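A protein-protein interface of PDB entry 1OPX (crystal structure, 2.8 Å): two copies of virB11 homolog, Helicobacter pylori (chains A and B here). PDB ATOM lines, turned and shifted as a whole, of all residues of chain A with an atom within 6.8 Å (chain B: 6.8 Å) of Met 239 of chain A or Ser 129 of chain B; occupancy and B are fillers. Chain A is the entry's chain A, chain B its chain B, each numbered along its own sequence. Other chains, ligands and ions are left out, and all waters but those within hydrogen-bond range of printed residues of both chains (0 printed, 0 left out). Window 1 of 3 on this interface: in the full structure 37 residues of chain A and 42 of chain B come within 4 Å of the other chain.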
ATOM      1  N   ARG A 200      -9.823  16.431  13.229  1.00  0.00           N
ATOM      2  CA  ARG A 200      -9.917  15.996  14.602  1.00  0.00           C
ATOM      3  C   ARG A 200     -11.427  16.003  14.861  1.00  0.00           C
ATOM      4  O   ARG A 200     -12.143  16.954  14.531  1.00  0.00           O
ATOM      5  CB  ARG A 200      -9.178  16.977  15.515  1.00  0.00           C
ATOM      6  CG  ARG A 200      -9.210  16.631  16.997  1.00  0.00           C
ATOM      7  CD  ARG A 200      -8.282  17.569  17.787  1.00  0.00           C
ATOM      8  NE  ARG A 200      -8.665  17.773  19.193  1.00  0.00           N
ATOM      9  CZ  ARG A 200      -8.507  16.878  20.164  1.00  0.00           C
ATOM     10  NH1 ARG A 200      -7.971  15.689  19.898  1.00  0.00           N
ATOM     11  NH2 ARG A 200      -8.872  17.181  21.404  1.00  0.00           N
ATOM     12  N   ILE A 202     -14.610  15.142  17.710  1.00  0.00           N
ATOM     13  CA  ILE A 202     -15.003  14.884  19.071  1.00  0.00           C
ATOM     14  C   ILE A 202     -16.448  14.436  18.955  1.00  0.00           C
ATOM     15  O   ILE A 202     -17.262  15.078  18.265  1.00  0.00           O
ATOM     16  CB  ILE A 202     -14.894  16.128  19.943  1.00  0.00           C
ATOM     17  CG1 ILE A 202     -13.462  16.661  19.859  1.00  0.00           C
ATOM     18  CG2 ILE A 202     -15.297  15.776  21.391  1.00  0.00           C
ATOM     19  CD1 ILE A 202     -13.072  17.606  20.973  1.00  0.00           C
ATOM     20  N   THR A 219     -11.635  12.007  19.969  1.00  0.00           N
ATOM     21  CA  THR A 219     -11.961  11.788  21.368  1.00  0.00           C
ATOM     22  C   THR A 219     -13.466  11.641  21.523  1.00  0.00           C
ATOM     23  O   THR A 219     -14.248  12.333  20.865  1.00  0.00           O
ATOM     24  CB  THR A 219     -11.487  12.973  22.221  1.00  0.00           C
ATOM     25  OG1 THR A 219     -10.054  12.968  22.284  1.00  0.00           O
ATOM     26  CG2 THR A 219     -12.070  12.900  23.625  1.00  0.00           C
ATOM     27  N   GLN A 220     -13.874  10.736  22.397  1.00  0.00           N
ATOM     28  CA  GLN A 220     -15.283  10.502  22.628  1.00  0.00           C
ATOM     29  C   GLN A 220     -15.663  10.955  24.015  1.00  0.00           C
ATOM     30  O   GLN A 220     -14.956  10.665  25.002  1.00  0.00           O
ATOM     31  CB  GLN A 220     -15.596   9.024  22.477  1.00  0.00           C
ATOM     32  CG  GLN A 220     -15.304   8.493  21.095  1.00  0.00           C
ATOM     33  CD  GLN A 220     -15.239   6.964  21.066  1.00  0.00           C
ATOM     34  OE1 GLN A 220     -14.347   6.363  21.677  1.00  0.00           O
ATOM     35  NE2 GLN A 220     -16.193   6.328  20.352  1.00  0.00           N
ATOM     36  N   LEU A 221     -16.780  11.674  24.077  1.00  0.00           N
ATOM     37  CA  LEU A 221     -17.314  12.180  25.329  1.00  0.00           C
ATOM     38  C   LEU A 221     -18.650  11.497  25.529  1.00  0.00           C
ATOM     39  O   LEU A 221     -19.369  11.235  24.558  1.00  0.00           O
ATOM     40  CB  LEU A 221     -17.513  13.692  25.244  1.00  0.00           C
ATOM     41  CG  LEU A 221     -16.266  14.484  24.822  1.00  0.00           C
ATOM     42  CD1 LEU A 221     -16.564  15.987  24.714  1.00  0.00           C
ATOM     43  CD2 LEU A 221     -15.170  14.216  25.845  1.00  0.00           C
ATOM     44  N   CYS A 232     -20.615  18.160  28.114  1.00  0.00           N
ATOM     45  CA  CYS A 232     -19.745  17.520  27.136  1.00  0.00           C
ATOM     46  C   CYS A 232     -19.578  18.376  25.884  1.00  0.00           C
ATOM     47  O   CYS A 232     -18.535  18.342  25.228  1.00  0.00           O
ATOM     48  CB  CYS A 232     -20.296  16.145  26.754  1.00  0.00           C
ATOM     49  SG  CYS A 232     -20.502  15.066  28.169  1.00  0.00           S
ATOM     50  N   LYS A 234     -19.827  21.611  26.049  1.00  0.00           N
ATOM     51  CA  LYS A 234     -19.111  22.770  26.553  1.00  0.00           C
ATOM     52  C   LYS A 234     -17.613  22.438  26.605  1.00  0.00           C
ATOM     53  O   LYS A 234     -16.775  23.257  26.262  1.00  0.00           O
ATOM     54  CB  LYS A 234     -19.616  23.150  27.946  1.00  0.00           C
ATOM     55  CG  LYS A 234     -18.836  24.303  28.553  1.00  0.00           C
ATOM     56  CD  LYS A 234     -19.238  24.599  30.002  1.00  0.00           C
ATOM     57  CE  LYS A 234     -18.380  25.729  30.606  1.00  0.00           C
ATOM     58  NZ  LYS A 234     -18.668  25.981  32.057  1.00  0.00           N
ATOM     59  N   SER A 235     -17.294  21.223  27.029  1.00  0.00           N
ATOM     60  CA  SER A 235     -15.916  20.772  27.113  1.00  0.00           C
ATOM     61  C   SER A 235     -15.408  20.654  25.691  1.00  0.00           C
ATOM     62  O   SER A 235     -14.299  21.067  25.369  1.00  0.00           O
ATOM     63  CB  SER A 235     -15.859  19.403  27.787  1.00  0.00           C
ATOM     64  OG  SER A 235     -14.581  19.158  28.343  1.00  0.00           O
ATOM     65  N   CYS A 236     -16.253  20.079  24.843  1.00  0.00           N
ATOM     66  CA  CYS A 236     -15.942  19.886  23.430  1.00  0.00           C
ATOM     67  C   CYS A 236     -15.338  21.143  22.809  1.00  0.00           C
ATOM     68  O   CYS A 236     -14.248  21.107  22.239  1.00  0.00           O
ATOM     69  CB  CYS A 236     -17.211  19.501  22.669  1.00  0.00           C
ATOM     70  SG  CYS A 236     -16.974  19.382  20.891  1.00  0.00           S
ATOM     71  N   LEU A 237     -16.051  22.255  22.932  1.00  0.00           N
ATOM     72  CA  LEU A 237     -15.577  23.518  22.387  1.00  0.00           C
ATOM     73  C   LEU A 237     -14.263  23.986  23.023  1.00  0.00           C
ATOM     74  O   LEU A 237     -13.743  25.035  22.651  1.00  0.00           O
ATOM     75  CB  LEU A 237     -16.663  24.598  22.527  1.00  0.00           C
ATOM     76  CG  LEU A 237     -17.943  24.291  21.745  1.00  0.00           C
ATOM     77  CD1 LEU A 237     -18.990  25.338  22.077  1.00  0.00           C
ATOM     78  CD2 LEU A 237     -17.663  24.253  20.241  1.00  0.00           C
ATOM     79  N   ARG A 238     -13.732  23.220  23.977  1.00  0.00           N
ATOM     80  CA  ARG A 238     -12.450  23.576  24.606  1.00  0.00           C
ATOM     81  C   ARG A 238     -11.376  22.518  24.300  1.00  0.00           C
ATOM     82  O   ARG A 238     -10.335  22.476  24.957  1.00  0.00           O
ATOM     83  CB  ARG A 238     -12.586  23.712  26.130  1.00  0.00           C
ATOM     84  CG  ARG A 238     -13.730  24.600  26.584  1.00  0.00           C
ATOM     85  CD  ARG A 238     -13.370  25.503  27.767  1.00  0.00           C
ATOM     86  NE  ARG A 238     -14.578  25.914  28.477  1.00  0.00           N
ATOM     87  CZ  ARG A 238     -14.632  26.854  29.416  1.00  0.00           C
ATOM     88  NH1 ARG A 238     -13.533  27.515  29.766  1.00  0.00           N
ATOM     89  NH2 ARG A 238     -15.788  27.109  30.020  1.00  0.00           N
ATOM     90  N   MET A 239     -11.640  21.685  23.292  1.00  0.00           N
ATOM     91  CA  MET A 239     -10.735  20.612  22.894  1.00  0.00           C
ATOM     92  C   MET A 239     -10.278  20.686  21.428  1.00  0.00           C
ATOM     93  O   MET A 239      -9.881  19.681  20.837  1.00  0.00           O
ATOM     94  CB  MET A 239     -11.413  19.278  23.193  1.00  0.00           C
ATOM     95  CG  MET A 239     -11.629  19.094  24.685  1.00  0.00           C
ATOM     96  SD  MET A 239     -13.039  17.893  25.172  1.00  0.00           S
ATOM     97  CE  MET A 239     -12.059  16.214  25.125  1.00  0.00           C
ATOM     98  N   ARG A 240     -10.330  21.888  20.857  1.00  0.00           N
ATOM     99  CA  ARG A 240      -9.915  22.141  19.472  1.00  0.00           C
ATOM    100  C   ARG A 240     -10.391  21.099  18.451  1.00  0.00           C
ATOM    101  O   ARG A 240      -9.587  20.463  17.768  1.00  0.00           O
ATOM    102  CB  ARG A 240      -8.389  22.255  19.402  1.00  0.00           C
ATOM    103  CG  ARG A 240      -7.879  22.737  18.057  1.00  0.00           C
ATOM    104  CD  ARG A 240      -8.148  24.221  17.842  1.00  0.00           C
ATOM    105  NE  ARG A 240      -7.201  25.026  18.594  1.00  0.00           N
ATOM    106  CZ  ARG A 240      -6.346  25.882  18.044  1.00  0.00           C
ATOM    107  NH1 ARG A 240      -6.320  26.060  16.728  1.00  0.00           N
ATOM    108  NH2 ARG A 240      -5.492  26.540  18.817  1.00  0.00           N
ATOM    109  N   PRO A 241     -11.713  20.924  18.329  1.00  0.00           N
ATOM    110  CA  PRO A 241     -12.286  19.957  17.386  1.00  0.00           C
ATOM    111  C   PRO A 241     -12.424  20.526  15.964  1.00  0.00           C
ATOM    112  O   PRO A 241     -12.612  21.722  15.786  1.00  0.00           O
ATOM    113  CB  PRO A 241     -13.644  19.667  18.012  1.00  0.00           C
ATOM    114  CG  PRO A 241     -14.044  21.045  18.500  1.00  0.00           C
ATOM    115  CD  PRO A 241     -12.765  21.529  19.171  1.00  0.00           C
ATOM    116  N   ASP A 242     -12.328  19.676  14.950  1.00  0.00           N
ATOM    117  CA  ASP A 242     -12.502  20.143  13.578  1.00  0.00           C
ATOM    118  C   ASP A 242     -13.945  19.841  13.210  1.00  0.00           C
ATOM    119  O   ASP A 242     -14.593  20.598  12.495  1.00  0.00           O
ATOM    120  CB  ASP A 242     -11.554  19.413  12.623  1.00  0.00           C
ATOM    121  CG  ASP A 242     -10.162  19.996  12.633  1.00  0.00           C
ATOM    122  OD1 ASP A 242      -9.984  21.151  12.207  1.00  0.00           O
ATOM    123  OD2 ASP A 242      -9.241  19.294  13.073  1.00  0.00           O
ATOM    124  N   GLU B  47      -1.927  24.185  19.547  1.00  0.00           N
ATOM    125  CA  GLU B  47      -2.636  23.337  20.501  1.00  0.00           C
ATOM    126  C   GLU B  47      -1.926  21.999  20.638  1.00  0.00           C
ATOM    127  O   GLU B  47      -1.473  21.421  19.647  1.00  0.00           O
ATOM    128  CB  GLU B  47      -4.068  23.087  20.009  1.00  0.00           C
ATOM    129  CG  GLU B  47      -5.011  22.386  20.998  1.00  0.00           C
ATOM    130  CD  GLU B  47      -5.872  23.371  21.804  1.00  0.00           C
ATOM    131  OE1 GLU B  47      -6.067  24.508  21.321  1.00  0.00           O
ATOM    132  OE2 GLU B  47      -6.372  23.005  22.902  1.00  0.00           O
ATOM    133  N   CYS B  49      -2.725  18.345  21.980  1.00  0.00           N
ATOM    134  CA  CYS B  49      -3.776  17.452  22.430  1.00  0.00           C
ATOM    135  C   CYS B  49      -3.256  16.070  22.762  1.00  0.00           C
ATOM    136  O   CYS B  49      -2.285  15.588  22.181  1.00  0.00           O
ATOM    137  CB  CYS B  49      -4.880  17.331  21.375  1.00  0.00           C
ATOM    138  SG  CYS B  49      -5.862  18.805  21.216  1.00  0.00           S
ATOM    139  N   TYR B  50      -3.886  15.449  23.742  1.00  0.00           N
ATOM    140  CA  TYR B  50      -3.546  14.094  24.103  1.00  0.00           C
ATOM    141  C   TYR B  50      -4.901  13.417  24.214  1.00  0.00           C
ATOM    142  O   TYR B  50      -5.812  13.918  24.887  1.00  0.00           O
ATOM    143  CB  TYR B  50      -2.794  14.019  25.413  1.00  0.00           C
ATOM    144  CG  TYR B  50      -2.421  12.597  25.713  1.00  0.00           C
ATOM    145  CD1 TYR B  50      -1.578  11.881  24.863  1.00  0.00           C
ATOM    146  CD2 TYR B  50      -2.956  11.940  26.813  1.00  0.00           C
ATOM    147  CE1 TYR B  50      -1.280  10.537  25.105  1.00  0.00           C
ATOM    148  CE2 TYR B  50      -2.668  10.586  27.071  1.00  0.00           C
ATOM    149  CZ  TYR B  50      -1.830   9.891  26.212  1.00  0.00           C
ATOM    150  OH  TYR B  50      -1.553   8.561  26.451  1.00  0.00           O
ATOM    151  N   ASN B  51      -5.042  12.290  23.528  1.00  0.00           N
ATOM    152  CA  ASN B  51      -6.315  11.598  23.490  1.00  0.00           C
ATOM    153  C   ASN B  51      -6.349  10.274  24.253  1.00  0.00           C
ATOM    154  O   ASN B  51      -7.130   9.372  23.942  1.00  0.00           O
ATOM    155  CB  ASN B  51      -6.702  11.452  22.021  1.00  0.00           C
ATOM    156  CG  ASN B  51      -6.637  12.803  21.273  1.00  0.00           C
ATOM    157  OD1 ASN B  51      -6.673  12.863  20.039  1.00  0.00           O
ATOM    158  ND2 ASN B  51      -6.550  13.892  22.034  1.00  0.00           N
ATOM    159  N   GLY B  52      -5.502  10.196  25.279  1.00  0.00           N
ATOM    160  CA  GLY B  52      -5.425   9.022  26.131  1.00  0.00           C
ATOM    161  C   GLY B  52      -5.117   7.746  25.391  1.00  0.00           C
ATOM    162  O   GLY B  52      -5.512   6.659  25.820  1.00  0.00           O
ATOM    163  N   TRP B  65      -2.078  18.705  11.538  1.00  0.00           N
ATOM    164  CA  TRP B  65      -2.049  17.925  12.780  1.00  0.00           C
ATOM    165  C   TRP B  65      -0.889  16.937  12.694  1.00  0.00           C
ATOM    166  O   TRP B  65      -0.818  16.155  11.745  1.00  0.00           O
ATOM    167  CB  TRP B  65      -3.343  17.122  12.985  1.00  0.00           C
ATOM    168  CG  TRP B  65      -4.522  17.900  13.560  1.00  0.00           C
ATOM    169  CD1 TRP B  65      -5.636  18.339  12.882  1.00  0.00           C
ATOM    170  CD2 TRP B  65      -4.688  18.343  14.922  1.00  0.00           C
ATOM    171  NE1 TRP B  65      -6.471  19.019  13.735  1.00  0.00           N
ATOM    172  CE2 TRP B  65      -5.917  19.044  14.989  1.00  0.00           C
ATOM    173  CE3 TRP B  65      -3.914  18.222  16.088  1.00  0.00           C
ATOM    174  CZ2 TRP B  65      -6.388  19.623  16.173  1.00  0.00           C
ATOM    175  CZ3 TRP B  65      -4.387  18.806  17.274  1.00  0.00           C
ATOM    176  CH2 TRP B  65      -5.610  19.496  17.299  1.00  0.00           C
ATOM    177  N   GLN B 115      -7.606  21.791  29.301  1.00  0.00           N
ATOM    178  CA  GLN B 115      -8.892  21.107  29.426  1.00  0.00           C
ATOM    179  C   GLN B 115      -8.667  19.612  29.633  1.00  0.00           C
ATOM    180  O   GLN B 115      -8.246  18.922  28.713  1.00  0.00           O
ATOM    181  CB  GLN B 115      -9.704  21.309  28.145  1.00  0.00           C
ATOM    182  CG  GLN B 115     -11.187  20.989  28.252  1.00  0.00           C
ATOM    183  CD  GLN B 115     -11.931  21.964  29.150  1.00  0.00           C
ATOM    184  OE1 GLN B 115     -11.650  23.156  29.153  1.00  0.00           O
ATOM    185  NE2 GLN B 115     -12.898  21.462  29.902  1.00  0.00           N
ATOM    186  N   ILE B 116      -8.957  19.098  30.820  1.00  0.00           N
ATOM    187  CA  ILE B 116      -8.770  17.670  31.074  1.00  0.00           C
ATOM    188  C   ILE B 116     -10.069  16.888  31.270  1.00  0.00           C
ATOM    189  O   ILE B 116     -10.974  17.332  31.973  1.00  0.00           O
ATOM    190  CB  ILE B 116      -7.913  17.437  32.320  1.00  0.00           C
ATOM    191  CG1 ILE B 116      -6.478  17.895  32.046  1.00  0.00           C
ATOM    192  CG2 ILE B 116      -8.000  15.949  32.747  1.00  0.00           C
ATOM    193  CD1 ILE B 116      -5.542  17.683  33.201  1.00  0.00           C
ATOM    194  N   VAL B 117     -10.158  15.714  30.664  1.00  0.00           N
ATOM    195  CA  VAL B 117     -11.354  14.918  30.821  1.00  0.00           C
ATOM    196  C   VAL B 117     -10.979  13.494  31.229  1.00  0.00           C
ATOM    197  O   VAL B 117     -10.104  12.863  30.631  1.00  0.00           O
ATOM    198  CB  VAL B 117     -12.208  14.940  29.523  1.00  0.00           C
ATOM    199  CG1 VAL B 117     -13.447  14.080  29.682  1.00  0.00           C
ATOM    200  CG2 VAL B 117     -12.647  16.351  29.228  1.00  0.00           C
ATOM    201  N   LEU B 118     -11.642  13.008  32.274  1.00  0.00           N
ATOM    202  CA  LEU B 118     -11.392  11.680  32.815  1.00  0.00           C
ATOM    203  C   LEU B 118     -12.619  10.787  32.699  1.00  0.00           C
ATOM    204  O   LEU B 118     -13.683  11.216  32.236  1.00  0.00           O
ATOM    205  CB  LEU B 118     -10.996  11.783  34.300  1.00  0.00           C
ATOM    206  CG  LEU B 118      -9.902  12.768  34.708  1.00  0.00           C
ATOM    207  CD1 LEU B 118      -9.732  12.740  36.201  1.00  0.00           C
ATOM    208  CD2 LEU B 118      -8.595  12.401  34.011  1.00  0.00           C
ATOM    209  N   THR B 122     -14.951   9.914  29.687  1.00  0.00           N
ATOM    210  CA  THR B 122     -14.191   9.417  28.551  1.00  0.00           C
ATOM    211  C   THR B 122     -14.657   7.980  28.278  1.00  0.00           C
ATOM    212  O   THR B 122     -15.332   7.369  29.117  1.00  0.00           O
ATOM    213  CB  THR B 122     -12.670   9.451  28.838  1.00  0.00           C
ATOM    214  OG1 THR B 122     -12.388   8.684  30.012  1.00  0.00           O
ATOM    215  CG2 THR B 122     -12.203  10.879  29.064  1.00  0.00           C
ATOM    216  N   THR B 127      -8.327   6.121  29.611  1.00  0.00           N
ATOM    217  CA  THR B 127      -8.374   7.283  28.747  1.00  0.00           C
ATOM    218  C   THR B 127      -8.384   8.560  29.574  1.00  0.00           C
ATOM    219  O   THR B 127      -9.213   8.742  30.471  1.00  0.00           O
ATOM    220  CB  THR B 127      -9.635   7.283  27.855  1.00  0.00           C
ATOM    221  OG1 THR B 127      -9.712   6.068  27.096  1.00  0.00           O
ATOM    222  CG2 THR B 127      -9.592   8.466  26.896  1.00  0.00           C
ATOM    223  N   ILE B 128      -7.441   9.441  29.274  1.00  0.00           N
ATOM    224  CA  ILE B 128      -7.351  10.719  29.955  1.00  0.00           C
ATOM    225  C   ILE B 128      -7.109  11.767  28.870  1.00  0.00           C
ATOM    226  O   ILE B 128      -5.995  11.895  28.356  1.00  0.00           O
ATOM    227  CB  ILE B 128      -6.204  10.720  30.979  1.00  0.00           C
ATOM    228  CG1 ILE B 128      -6.468   9.645  32.044  1.00  0.00           C
ATOM    229  CG2 ILE B 128      -6.071  12.097  31.611  1.00  0.00           C
ATOM    230  CD1 ILE B 128      -5.477   9.644  33.180  1.00  0.00           C
ATOM    231  N   SER B 129      -8.169  12.489  28.507  1.00  0.00           N
ATOM    232  CA  SER B 129      -8.103  13.526  27.477  1.00  0.00           C
ATOM    233  C   SER B 129      -7.528  14.856  27.965  1.00  0.00           C
ATOM    234  O   SER B 129      -7.967  15.394  28.979  1.00  0.00           O
ATOM    235  CB  SER B 129      -9.486  13.775  26.909  1.00  0.00           C
ATOM    236  OG  SER B 129      -9.436  14.871  26.032  1.00  0.00           O
ATOM    237  N   ILE B 130      -6.558  15.390  27.225  1.00  0.00           N
ATOM    238  CA  ILE B 130      -5.917  16.655  27.588  1.00  0.00           C
ATOM    239  C   ILE B 130      -5.748  17.535  26.370  1.00  0.00           C
ATOM    240  O   ILE B 130      -5.283  17.067  25.330  1.00  0.00           O
ATOM    241  CB  ILE B 130      -4.513  16.447  28.189  1.00  0.00           C
ATOM    242  CG1 ILE B 130      -4.579  15.517  29.408  1.00  0.00           C
ATOM    243  CG2 ILE B 130      -3.940  17.795  28.610  1.00  0.00           C
ATOM    244  CD1 ILE B 130      -3.231  15.160  29.969  1.00  0.00           C
ATOM    245  N   SER B 131      -6.110  18.811  26.507  1.00  0.00           N
ATOM    246  CA  SER B 131      -6.016  19.773  25.417  1.00  0.00           C
ATOM    247  C   SER B 131      -5.388  21.080  25.878  1.00  0.00           C
ATOM    248  O   SER B 131      -6.007  21.847  26.628  1.00  0.00           O
ATOM    249  CB  SER B 131      -7.398  20.048  24.877  1.00  0.00           C
ATOM    250  OG  SER B 131      -7.942  18.857  24.370  1.00  0.00           O
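Among the printed residues, pairs that only touch across the chains: Arg 200 of chain A with Trp 65 of chain B (3.2 Å), Arg 200 of chain A with Ser 131 of chain B (3.5 Å), Thr 219 of chain A with Asn 51 of chain B (3.6 Å), Gln 220 of chain A with Thr 122 of chain B (3.8 Å), Ser 235 of chain A with Val 117 of chain B (3.5 Å), Arg 238 of chain A with Gln 115 of chain B (3.2 Å), Arg 238 of chain A with Ser 131 of chain B (3.8 Å), Met 239 of chain A with Ser 129 of chain B (3.1 Å), Met 239 of chain A with Ser 131 of chain B (3.6 Å) and Arg 240 of chain A with Trp 65 of chain B (3.7 Å).
Hydrophobic or aromatic side chains of chain B that line the printed part of chain A: Trp 65 and Val 117.
Along chain B the printed residues that touch a printed residue of chain A span positions 47 to 131.
Hydrophobic or aromatic side chains of chain A within 4 Å of the printed part of chain B: Met 239.
Among the printed residues, 15 pairs touch across the chains.
No position is printed for both chains.
Of the 15 pairs that touch across the chains among the printed residues, none has its exchanged pair printed and touching as well.
Met 239 of chain A touches just these residues of chain B: Ser 129 (3.1 Å) and Ser 131 (3.6 Å).
Ser 129 of chain B touches just one residue of chain A: Met 239 (3.1 Å).
Of the printed residues of chain A, Ser 131 of chain B touches Arg 200, Arg 238 and Met 239.
Printed residues of chain A within 4 Å of Trp 65 of chain B: Arg 200 (3.2 Å), Arg 240 (3.7 Å) and Asp 242 (2.9 Å).
Of the printed residues of chain B, Ser 235 of chain A touches Gln 115 and Val 117.
Of the printed residues of chain B, Thr 219 of chain A touches Asn 51 (3.6 Å).
Of the printed residues of chain A, Asn 51 of chain B touches Arg 200 and Thr 219.
NE1 of Trp 65 of chain B lies within hydrogen-bond range of OD2 of Asp 242 of chain A, at 2.9 Å.
The guanidinium group (NH1) of Arg 200 of chain A sits at hydrogen-bond distance from the side-chain amide oxygen (OD1) of Asn 51 of chain B (3.1 Å).
The guanidinium group (NE) of Arg 240 of chain A lies within salt-bridge range of the side-chain carboxylate (OE1) of Glu 47 of chain B, 3.0 Å away.
The side-chain hydroxyl of Ser 235 of chain A is in hydrogen-bond range of the side-chain amide nitrogen of Gln 115 of chain B, 3.3 Å away.
NH2 of Arg 200 of chain A is in hydrogen-bond range of SG of Cys 49 of chain B (3.4 Å).
The backbone NH (N) of Ser 131 of chain B lies within hydrogen-bond range of the backbone carbonyl oxygen (O) of Gln 115 of chain B (3.1 Å).
The guanidinium group of Arg 200 of chain A lies within hydrogen-bond range of the backbone carbonyl oxygen of Met 239 of chain A, at 2.8 Å.
The side-chain hydroxyl (OG) of Ser 235 of chain A sits close to the side-chain sulfur (SD) of Met 239 of chain A (3.7 Å).
The backbone carbonyl oxygen (O) of Arg 240 of chain A lies close to the guanidinium group (NE) of Arg 200 of chain A, 3.2 Å away.
The side-chain hydroxyl (OG1) of Thr 122 of chain B is in hydrogen-bond range of the backbone carbonyl oxygen (O) of Thr 127 of chain B (3.2 Å).
The backbone NH (N) of Val 117 of chain B sits at hydrogen-bond distance from the backbone carbonyl oxygen (O) of Ser 129 of chain B (2.8 Å).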
